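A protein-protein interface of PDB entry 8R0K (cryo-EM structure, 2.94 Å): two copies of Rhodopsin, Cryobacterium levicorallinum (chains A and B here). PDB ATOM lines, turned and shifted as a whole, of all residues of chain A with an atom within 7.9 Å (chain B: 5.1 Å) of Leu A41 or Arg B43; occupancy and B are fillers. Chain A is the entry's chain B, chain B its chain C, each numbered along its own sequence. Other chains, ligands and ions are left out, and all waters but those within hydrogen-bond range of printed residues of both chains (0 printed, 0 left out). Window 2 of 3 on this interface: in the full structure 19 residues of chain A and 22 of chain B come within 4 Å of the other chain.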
ATOM      1  N   PHE A  34      34.163  -8.458  28.155  1.00  0.00           N
ATOM      2  CA  PHE A  34      33.016  -7.587  28.266  1.00  0.00           C
ATOM      3  C   PHE A  34      33.451  -6.217  28.757  1.00  0.00           C
ATOM      4  O   PHE A  34      32.937  -5.214  28.281  1.00  0.00           O
ATOM      5  CB  PHE A  34      32.019  -8.171  29.246  1.00  0.00           C
ATOM      6  CG  PHE A  34      30.966  -7.200  29.669  1.00  0.00           C
ATOM      7  CD1 PHE A  34      30.887  -6.785  30.983  1.00  0.00           C
ATOM      8  CD2 PHE A  34      30.053  -6.718  28.754  1.00  0.00           C
ATOM      9  CE1 PHE A  34      29.886  -5.913  31.382  1.00  0.00           C
ATOM     10  CE2 PHE A  34      29.037  -5.875  29.160  1.00  0.00           C
ATOM     11  CZ  PHE A  34      28.961  -5.469  30.472  1.00  0.00           C
ATOM     12  N   GLY A  35      34.378  -6.202  29.719  1.00  0.00           N
ATOM     13  CA  GLY A  35      34.954  -4.981  30.250  1.00  0.00           C
ATOM     14  C   GLY A  35      35.625  -4.144  29.168  1.00  0.00           C
ATOM     15  O   GLY A  35      35.604  -2.919  29.240  1.00  0.00           O
ATOM     16  N   LEU A  36      36.222  -4.802  28.182  1.00  0.00           N
ATOM     17  CA  LEU A  36      36.838  -4.092  27.087  1.00  0.00           C
ATOM     18  C   LEU A  36      35.732  -3.468  26.248  1.00  0.00           C
ATOM     19  O   LEU A  36      35.806  -2.285  25.908  1.00  0.00           O
ATOM     20  CB  LEU A  36      37.721  -5.055  26.291  1.00  0.00           C
ATOM     21  CG  LEU A  36      38.537  -4.420  25.171  1.00  0.00           C
ATOM     22  CD1 LEU A  36      39.384  -3.252  25.668  1.00  0.00           C
ATOM     23  CD2 LEU A  36      39.434  -5.438  24.531  1.00  0.00           C
ATOM     24  N   ALA A  37      34.687  -4.233  25.961  1.00  0.00           N
ATOM     25  CA  ALA A  37      33.641  -3.718  25.102  1.00  0.00           C
ATOM     26  C   ALA A  37      32.865  -2.593  25.783  1.00  0.00           C
ATOM     27  O   ALA A  37      32.420  -1.669  25.112  1.00  0.00           O
ATOM     28  CB  ALA A  37      32.722  -4.822  24.706  1.00  0.00           C
ATOM     29  N   ARG A  38      32.647  -2.695  27.089  1.00  0.00           N
ATOM     30  CA  ARG A  38      32.003  -1.636  27.834  1.00  0.00           C
ATOM     31  C   ARG A  38      32.853  -0.383  27.680  1.00  0.00           C
ATOM     32  O   ARG A  38      32.327   0.692  27.401  1.00  0.00           O
ATOM     33  CB  ARG A  38      31.828  -2.071  29.289  1.00  0.00           C
ATOM     34  CG  ARG A  38      31.261  -0.991  30.181  1.00  0.00           C
ATOM     35  CD  ARG A  38      30.263  -1.434  31.232  1.00  0.00           C
ATOM     36  NE  ARG A  38      30.821  -1.516  32.569  1.00  0.00           N
ATOM     37  CZ  ARG A  38      31.639  -2.484  32.968  1.00  0.00           C
ATOM     38  NH1 ARG A  38      31.875  -3.502  32.154  1.00  0.00           N
ATOM     39  NH2 ARG A  38      32.226  -2.425  34.163  1.00  0.00           N
ATOM     40  N   THR A  39      34.172  -0.533  27.821  1.00  0.00           N
ATOM     41  CA  THR A  39      35.081   0.597  27.808  1.00  0.00           C
ATOM     42  C   THR A  39      34.973   1.334  26.481  1.00  0.00           C
ATOM     43  O   THR A  39      34.858   2.553  26.481  1.00  0.00           O
ATOM     44  CB  THR A  39      36.525   0.165  28.068  1.00  0.00           C
ATOM     45  OG1 THR A  39      36.596  -0.431  29.356  1.00  0.00           O
ATOM     46  CG2 THR A  39      37.508   1.315  28.053  1.00  0.00           C
ATOM     47  N   TRP A  40      34.990   0.602  25.368  1.00  0.00           N
ATOM     48  CA  TRP A  40      34.933   1.235  24.065  1.00  0.00           C
ATOM     49  C   TRP A  40      33.551   1.857  23.831  1.00  0.00           C
ATOM     50  O   TRP A  40      33.454   2.923  23.238  1.00  0.00           O
ATOM     51  CB  TRP A  40      35.299   0.238  22.964  1.00  0.00           C
ATOM     52  CG  TRP A  40      35.924   0.881  21.758  1.00  0.00           C
ATOM     53  CD1 TRP A  40      35.296   1.436  20.674  1.00  0.00           C
ATOM     54  CD2 TRP A  40      37.341   1.095  21.556  1.00  0.00           C
ATOM     55  NE1 TRP A  40      36.217   1.946  19.799  1.00  0.00           N
ATOM     56  CE2 TRP A  40      37.478   1.748  20.307  1.00  0.00           C
ATOM     57  CE3 TRP A  40      38.496   0.787  22.293  1.00  0.00           C
ATOM     58  CZ2 TRP A  40      38.723   2.108  19.793  1.00  0.00           C
ATOM     59  CZ3 TRP A  40      39.730   1.122  21.773  1.00  0.00           C
ATOM     60  CH2 TRP A  40      39.836   1.782  20.542  1.00  0.00           C
ATOM     61  N   LEU A  41      32.477   1.244  24.302  1.00  0.00           N
ATOM     62  CA  LEU A  41      31.165   1.781  23.994  1.00  0.00           C
ATOM     63  C   LEU A  41      30.866   3.024  24.832  1.00  0.00           C
ATOM     64  O   LEU A  41      29.924   3.755  24.532  1.00  0.00           O
ATOM     65  CB  LEU A  41      30.101   0.716  24.232  1.00  0.00           C
ATOM     66  CG  LEU A  41      30.128  -0.455  23.273  1.00  0.00           C
ATOM     67  CD1 LEU A  41      29.192  -1.551  23.763  1.00  0.00           C
ATOM     68  CD2 LEU A  41      29.726  -0.012  21.886  1.00  0.00           C
ATOM     69  N   THR A  42      31.633   3.268  25.884  1.00  0.00           N
ATOM     70  CA  THR A  42      31.290   4.352  26.788  1.00  0.00           C
ATOM     71  C   THR A  42      32.472   5.308  26.952  1.00  0.00           C
ATOM     72  O   THR A  42      32.632   5.930  27.998  1.00  0.00           O
ATOM     73  CB  THR A  42      30.833   3.771  28.135  1.00  0.00           C
ATOM     74  OG1 THR A  42      31.873   3.024  28.768  1.00  0.00           O
ATOM     75  CG2 THR A  42      29.638   2.854  28.003  1.00  0.00           C
ATOM     76  N   ARG A  43      33.312   5.420  25.916  1.00  0.00           N
ATOM     77  CA  ARG A  43      34.531   6.217  25.997  1.00  0.00           C
ATOM     78  C   ARG A  43      34.207   7.687  25.750  1.00  0.00           C
ATOM     79  O   ARG A  43      35.034   8.556  25.987  1.00  0.00           O
ATOM     80  CB  ARG A  43      35.585   5.712  25.005  1.00  0.00           C
ATOM     81  CG  ARG A  43      35.086   5.578  23.575  1.00  0.00           C
ATOM     82  CD  ARG A  43      35.969   4.737  22.700  1.00  0.00           C
ATOM     83  NE  ARG A  43      36.950   5.578  22.069  1.00  0.00           N
ATOM     84  CZ  ARG A  43      37.025   5.768  20.759  1.00  0.00           C
ATOM     85  NH1 ARG A  43      36.179   5.141  19.952  1.00  0.00           N
ATOM     86  NH2 ARG A  43      37.954   6.584  20.268  1.00  0.00           N
ATOM     87  N   GLY A  44      33.003   7.951  25.236  1.00  0.00           N
ATOM     88  CA  GLY A  44      32.599   9.294  24.867  1.00  0.00           C
ATOM     89  C   GLY A  44      32.070  10.079  26.059  1.00  0.00           C
ATOM     90  O   GLY A  44      31.887  11.290  25.963  1.00  0.00           O
ATOM     91  N   GLU A  45      31.854   9.391  27.180  1.00  0.00           N
ATOM     92  CA  GLU A  45      31.215  10.012  28.324  1.00  0.00           C
ATOM     93  C   GLU A  45      32.239  10.807  29.129  1.00  0.00           C
ATOM     94  O   GLU A  45      31.853  11.547  30.036  1.00  0.00           O
ATOM     95  CB  GLU A  45      30.542   8.938  29.180  1.00  0.00           C
ATOM     96  CG  GLU A  45      29.470   8.162  28.424  1.00  0.00           C
ATOM     97  CD  GLU A  45      28.804   7.027  29.198  1.00  0.00           C
ATOM     98  OE1 GLU A  45      27.764   6.498  28.710  1.00  0.00           O
ATOM     99  OE2 GLU A  45      29.326   6.656  30.287  1.00  0.00           O
ATOM    100  N   HIS A 249      35.630   5.502  36.075  1.00  0.00           N
ATOM    101  CA  HIS A 249      34.888   6.131  34.998  1.00  0.00           C
ATOM    102  C   HIS A 249      33.754   6.964  35.561  1.00  0.00           C
ATOM    103  O   HIS A 249      33.439   8.002  35.004  1.00  0.00           O
ATOM    104  CB  HIS A 249      34.281   5.065  34.106  1.00  0.00           C
ATOM    105  CG  HIS A 249      33.465   5.559  32.994  1.00  0.00           C
ATOM    106  ND1 HIS A 249      33.997   5.960  31.792  1.00  0.00           N
ATOM    107  CD2 HIS A 249      32.131   5.588  32.855  1.00  0.00           C
ATOM    108  CE1 HIS A 249      32.999   6.268  30.970  1.00  0.00           C
ATOM    109  NE2 HIS A 249      31.851   6.047  31.589  1.00  0.00           N
ATOM    110  N   ARG B  38      24.916  -6.693  14.180  1.00  0.00           N
ATOM    111  CA  ARG B  38      23.693  -5.920  14.183  1.00  0.00           C
ATOM    112  C   ARG B  38      23.800  -4.894  15.303  1.00  0.00           C
ATOM    113  O   ARG B  38      23.506  -3.716  15.097  1.00  0.00           O
ATOM    114  CB  ARG B  38      22.497  -6.859  14.342  1.00  0.00           C
ATOM    115  CG  ARG B  38      21.173  -6.142  14.460  1.00  0.00           C
ATOM    116  CD  ARG B  38      19.996  -6.780  13.747  1.00  0.00           C
ATOM    117  NE  ARG B  38      19.088  -7.490  14.623  1.00  0.00           N
ATOM    118  CZ  ARG B  38      19.367  -8.665  15.179  1.00  0.00           C
ATOM    119  NH1 ARG B  38      20.474  -9.299  14.821  1.00  0.00           N
ATOM    120  NH2 ARG B  38      18.549  -9.199  16.085  1.00  0.00           N
ATOM    121  N   THR B  39      24.262  -5.336  16.474  1.00  0.00           N
ATOM    122  CA  THR B  39      24.306  -4.490  17.652  1.00  0.00           C
ATOM    123  C   THR B  39      25.186  -3.279  17.385  1.00  0.00           C
ATOM    124  O   THR B  39      24.780  -2.162  17.682  1.00  0.00           O
ATOM    125  CB  THR B  39      24.805  -5.255  18.881  1.00  0.00           C
ATOM    126  OG1 THR B  39      23.903  -6.319  19.151  1.00  0.00           O
ATOM    127  CG2 THR B  39      24.880  -4.403  20.127  1.00  0.00           C
ATOM    128  N   TRP B  40      26.367  -3.497  16.816  1.00  0.00           N
ATOM    129  CA  TRP B  40      27.281  -2.400  16.570  1.00  0.00           C
ATOM    130  C   TRP B  40      26.756  -1.479  15.474  1.00  0.00           C
ATOM    131  O   TRP B  40      26.916  -0.272  15.564  1.00  0.00           O
ATOM    132  CB  TRP B  40      28.675  -2.926  16.224  1.00  0.00           C
ATOM    133  CG  TRP B  40      29.769  -2.068  16.787  1.00  0.00           C
ATOM    134  CD1 TRP B  40      30.377  -0.996  16.205  1.00  0.00           C
ATOM    135  CD2 TRP B  40      30.369  -2.224  18.098  1.00  0.00           C
ATOM    136  NE1 TRP B  40      31.322  -0.473  17.060  1.00  0.00           N
ATOM    137  CE2 TRP B  40      31.336  -1.200  18.225  1.00  0.00           C
ATOM    138  CE3 TRP B  40      30.189  -3.134  19.156  1.00  0.00           C
ATOM    139  CZ2 TRP B  40      32.121  -1.075  19.372  1.00  0.00           C
ATOM    140  CZ3 TRP B  40      30.972  -3.013  20.282  1.00  0.00           C
ATOM    141  CH2 TRP B  40      31.926  -1.997  20.384  1.00  0.00           C
ATOM    142  N   LEU B  41      26.080  -2.009  14.459  1.00  0.00           N
ATOM    143  CA  LEU B  41      25.652  -1.153  13.372  1.00  0.00           C
ATOM    144  C   LEU B  41      24.443  -0.313  13.779  1.00  0.00           C
ATOM    145  O   LEU B  41      24.102   0.645  13.088  1.00  0.00           O
ATOM    146  CB  LEU B  41      25.321  -1.997  12.149  1.00  0.00           C
ATOM    147  CG  LEU B  41      26.504  -2.667  11.484  1.00  0.00           C
ATOM    148  CD1 LEU B  41      26.018  -3.661  10.439  1.00  0.00           C
ATOM    149  CD2 LEU B  41      27.401  -1.633  10.841  1.00  0.00           C
ATOM    150  N   THR B  42      23.773  -0.663  14.867  1.00  0.00           N
ATOM    151  CA  THR B  42      22.530   0.012  15.193  1.00  0.00           C
ATOM    152  C   THR B  42      22.584   0.579  16.612  1.00  0.00           C
ATOM    153  O   THR B  42      21.561   0.694  17.278  1.00  0.00           O
ATOM    154  CB  THR B  42      21.352  -0.957  15.010  1.00  0.00           C
ATOM    155  OG1 THR B  42      21.451  -2.081  15.886  1.00  0.00           O
ATOM    156  CG2 THR B  42      21.254  -1.496  13.602  1.00  0.00           C
ATOM    157  N   ARG B  43      23.787   0.929  17.083  1.00  0.00           N
ATOM    158  CA  ARG B  43      23.973   1.381  18.456  1.00  0.00           C
ATOM    159  C   ARG B  43      23.627   2.863  18.571  1.00  0.00           C
ATOM    160  O   ARG B  43      23.510   3.395  19.668  1.00  0.00           O
ATOM    161  CB  ARG B  43      25.406   1.116  18.924  1.00  0.00           C
ATOM    162  CG  ARG B  43      26.480   1.656  17.997  1.00  0.00           C
ATOM    163  CD  ARG B  43      27.837   1.071  18.273  1.00  0.00           C
ATOM    164  NE  ARG B  43      28.530   1.918  19.208  1.00  0.00           N
ATOM    165  CZ  ARG B  43      29.622   2.610  18.917  1.00  0.00           C
ATOM    166  NH1 ARG B  43      30.178   2.485  17.719  1.00  0.00           N
ATOM    167  NH2 ARG B  43      30.164   3.402  19.836  1.00  0.00           N
ATOM    168  N   GLY B  44      23.493   3.530  17.423  1.00  0.00           N
ATOM    169  CA  GLY B  44      23.243   4.959  17.384  1.00  0.00           C
ATOM    170  C   GLY B  44      21.766   5.287  17.550  1.00  0.00           C
ATOM    171  O   GLY B  44      21.409   6.446  17.752  1.00  0.00           O
ATOM    172  N   GLU B  45      20.917   4.264  17.488  1.00  0.00           N
ATOM    173  CA  GLU B  45      19.482   4.479  17.504  1.00  0.00           C
ATOM    174  C   GLU B  45      18.996   4.652  18.939  1.00  0.00           C
ATOM    175  O   GLU B  45      17.839   5.001  19.145  1.00  0.00           O
ATOM    176  CB  GLU B  45      18.777   3.317  16.803  1.00  0.00           C
ATOM    177  CG  GLU B  45      19.215   3.138  15.353  1.00  0.00           C
ATOM    178  CD  GLU B  45      18.633   1.937  14.617  1.00  0.00           C
ATOM    179  OE1 GLU B  45      18.799   1.860  13.369  1.00  0.00           O
ATOM    180  OE2 GLU B  45      18.022   1.067  15.286  1.00  0.00           O
ATOM    181  N   VAL B  46      19.882   4.424  19.915  1.00  0.00           N
ATOM    182  CA  VAL B  46      19.512   4.403  21.320  1.00  0.00           C
ATOM    183  C   VAL B  46      20.189   5.605  21.976  1.00  0.00           C
ATOM    184  O   VAL B  46      21.348   5.881  21.670  1.00  0.00           O
ATOM    185  CB  VAL B  46      19.921   3.049  21.943  1.00  0.00           C
ATOM    186  CG1 VAL B  46      19.779   2.979  23.452  1.00  0.00           C
ATOM    187  CG2 VAL B  46      19.125   1.909  21.355  1.00  0.00           C
ATOM    188  N   ARG B  51      22.028   3.480  27.245  1.00  0.00           N
ATOM    189  CA  ARG B  51      23.223   2.924  26.628  1.00  0.00           C
ATOM    190  C   ARG B  51      23.616   1.623  27.326  1.00  0.00           C
ATOM    191  O   ARG B  51      24.328   0.794  26.758  1.00  0.00           O
ATOM    192  CB  ARG B  51      24.378   3.923  26.672  1.00  0.00           C
ATOM    193  CG  ARG B  51      25.627   3.432  25.956  1.00  0.00           C
ATOM    194  CD  ARG B  51      26.685   4.497  25.835  1.00  0.00           C
ATOM    195  NE  ARG B  51      26.192   5.674  25.135  1.00  0.00           N
ATOM    196  CZ  ARG B  51      26.862   6.815  25.026  1.00  0.00           C
ATOM    197  NH1 ARG B  51      28.105   6.910  25.477  1.00  0.00           N
ATOM    198  NH2 ARG B  51      26.286   7.851  24.440  1.00  0.00           N
ATOM    199  N   VAL B  54      22.851  -1.137  25.226  1.00  0.00           N
ATOM    200  CA  VAL B  54      23.783  -1.422  24.152  1.00  0.00           C
ATOM    201  C   VAL B  54      24.961  -2.198  24.711  1.00  0.00           C
ATOM    202  O   VAL B  54      25.509  -3.068  24.042  1.00  0.00           O
ATOM    203  CB  VAL B  54      24.285  -0.133  23.491  1.00  0.00           C
ATOM    204  CG1 VAL B  54      25.311  -0.432  22.409  1.00  0.00           C
ATOM    205  CG2 VAL B  54      23.124   0.676  22.940  1.00  0.00           C
ATOM    206  N   VAL B  55      25.378  -1.807  25.915  1.00  0.00           N
ATOM    207  CA  VAL B  55      26.556  -2.380  26.522  1.00  0.00           C
ATOM    208  C   VAL B  55      26.249  -3.822  26.867  1.00  0.00           C
ATOM    209  O   VAL B  55      27.020  -4.702  26.503  1.00  0.00           O
ATOM    210  CB  VAL B  55      27.012  -1.555  27.731  1.00  0.00           C
ATOM    211  CG1 VAL B  55      28.062  -2.261  28.564  1.00  0.00           C
ATOM    212  CG2 VAL B  55      27.533  -0.214  27.255  1.00  0.00           C
ATOM    213  N   SER B  58      25.910  -6.053  23.789  1.00  0.00           N
ATOM    214  CA  SER B  58      27.184  -6.326  23.159  1.00  0.00           C
ATOM    215  C   SER B  58      27.896  -7.411  23.944  1.00  0.00           C
ATOM    216  O   SER B  58      28.355  -8.408  23.401  1.00  0.00           O
ATOM    217  CB  SER B  58      28.020  -5.080  23.064  1.00  0.00           C
ATOM    218  OG  SER B  58      27.465  -4.132  22.143  1.00  0.00           O
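Leu A41 touches Trp B40, but with the chains exchanged Trp A40 does not touch Leu B41 (11.6 Å). Leu A41 touches Arg B43, but with the chains exchanged Arg A43 does not touch Leu B41 (13.5 Å). Positions printed for both chains: 38, 39, 40, 41, 42, 43, 44 and 45. Of the 10 pairs that touch across the chains among the printed residues, none has its exchanged pair printed and touching as well.
Among the printed residues, pairs that only touch across the chains: Phe A34 with Val B55 (3.5 Å), Arg A38 with Val B55 (3.6 Å), Leu A41 with Trp B40 (3.3 Å), Leu A41 with Arg B43 (3.5 Å), Leu A41 with Arg B51 (3.6 Å), Leu A41 with Val B54 (3.99 Å), Leu A41 with Val B55 (3.9 Å), Leu A41 with Ser B58 (3.5 Å) and Thr A42 with Val B55 (3.8 Å).
Of the printed residues of chain B, Phe A34 touches Val B55 (3.5 Å). Of the printed residues of chain B, Arg A38 touches Val B55. Arg B43 touches just one residue of chain A: Leu A41. The nearest printed residue of chain B that does not touch Leu A41 is Thr B39 (6.3 Å). The nearest printed residue of chain B that does not touch Arg A38 is Ser B58 (6.6 Å).
NH1 of Arg B51 is in salt-bridge range of OE1 of Glu A45, at 3.3 Å.
The backbone carbonyl oxygen (O) of Arg A38 sits at hydrogen-bond distance from the side-chain hydroxyl (OG1) of Thr A42, 2.7 Å away. OE2 of Glu A45 sits at hydrogen-bond distance from NE2 of His A249 (2.9 Å). The backbone carbonyl oxygen of Val B54 lies within hydrogen-bond range of the side-chain hydroxyl of Ser B58 (2.9 Å).
Hydrophobic or aromatic side chains of chain B that line the printed part of chain A: Trp B40 and Val B55. Among the printed residues, Asp or Glu carboxylates within 4 Å of a Lys or Arg side-chain nitrogen of the other chain: Glu A45 with Arg B51 (3.3 Å).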
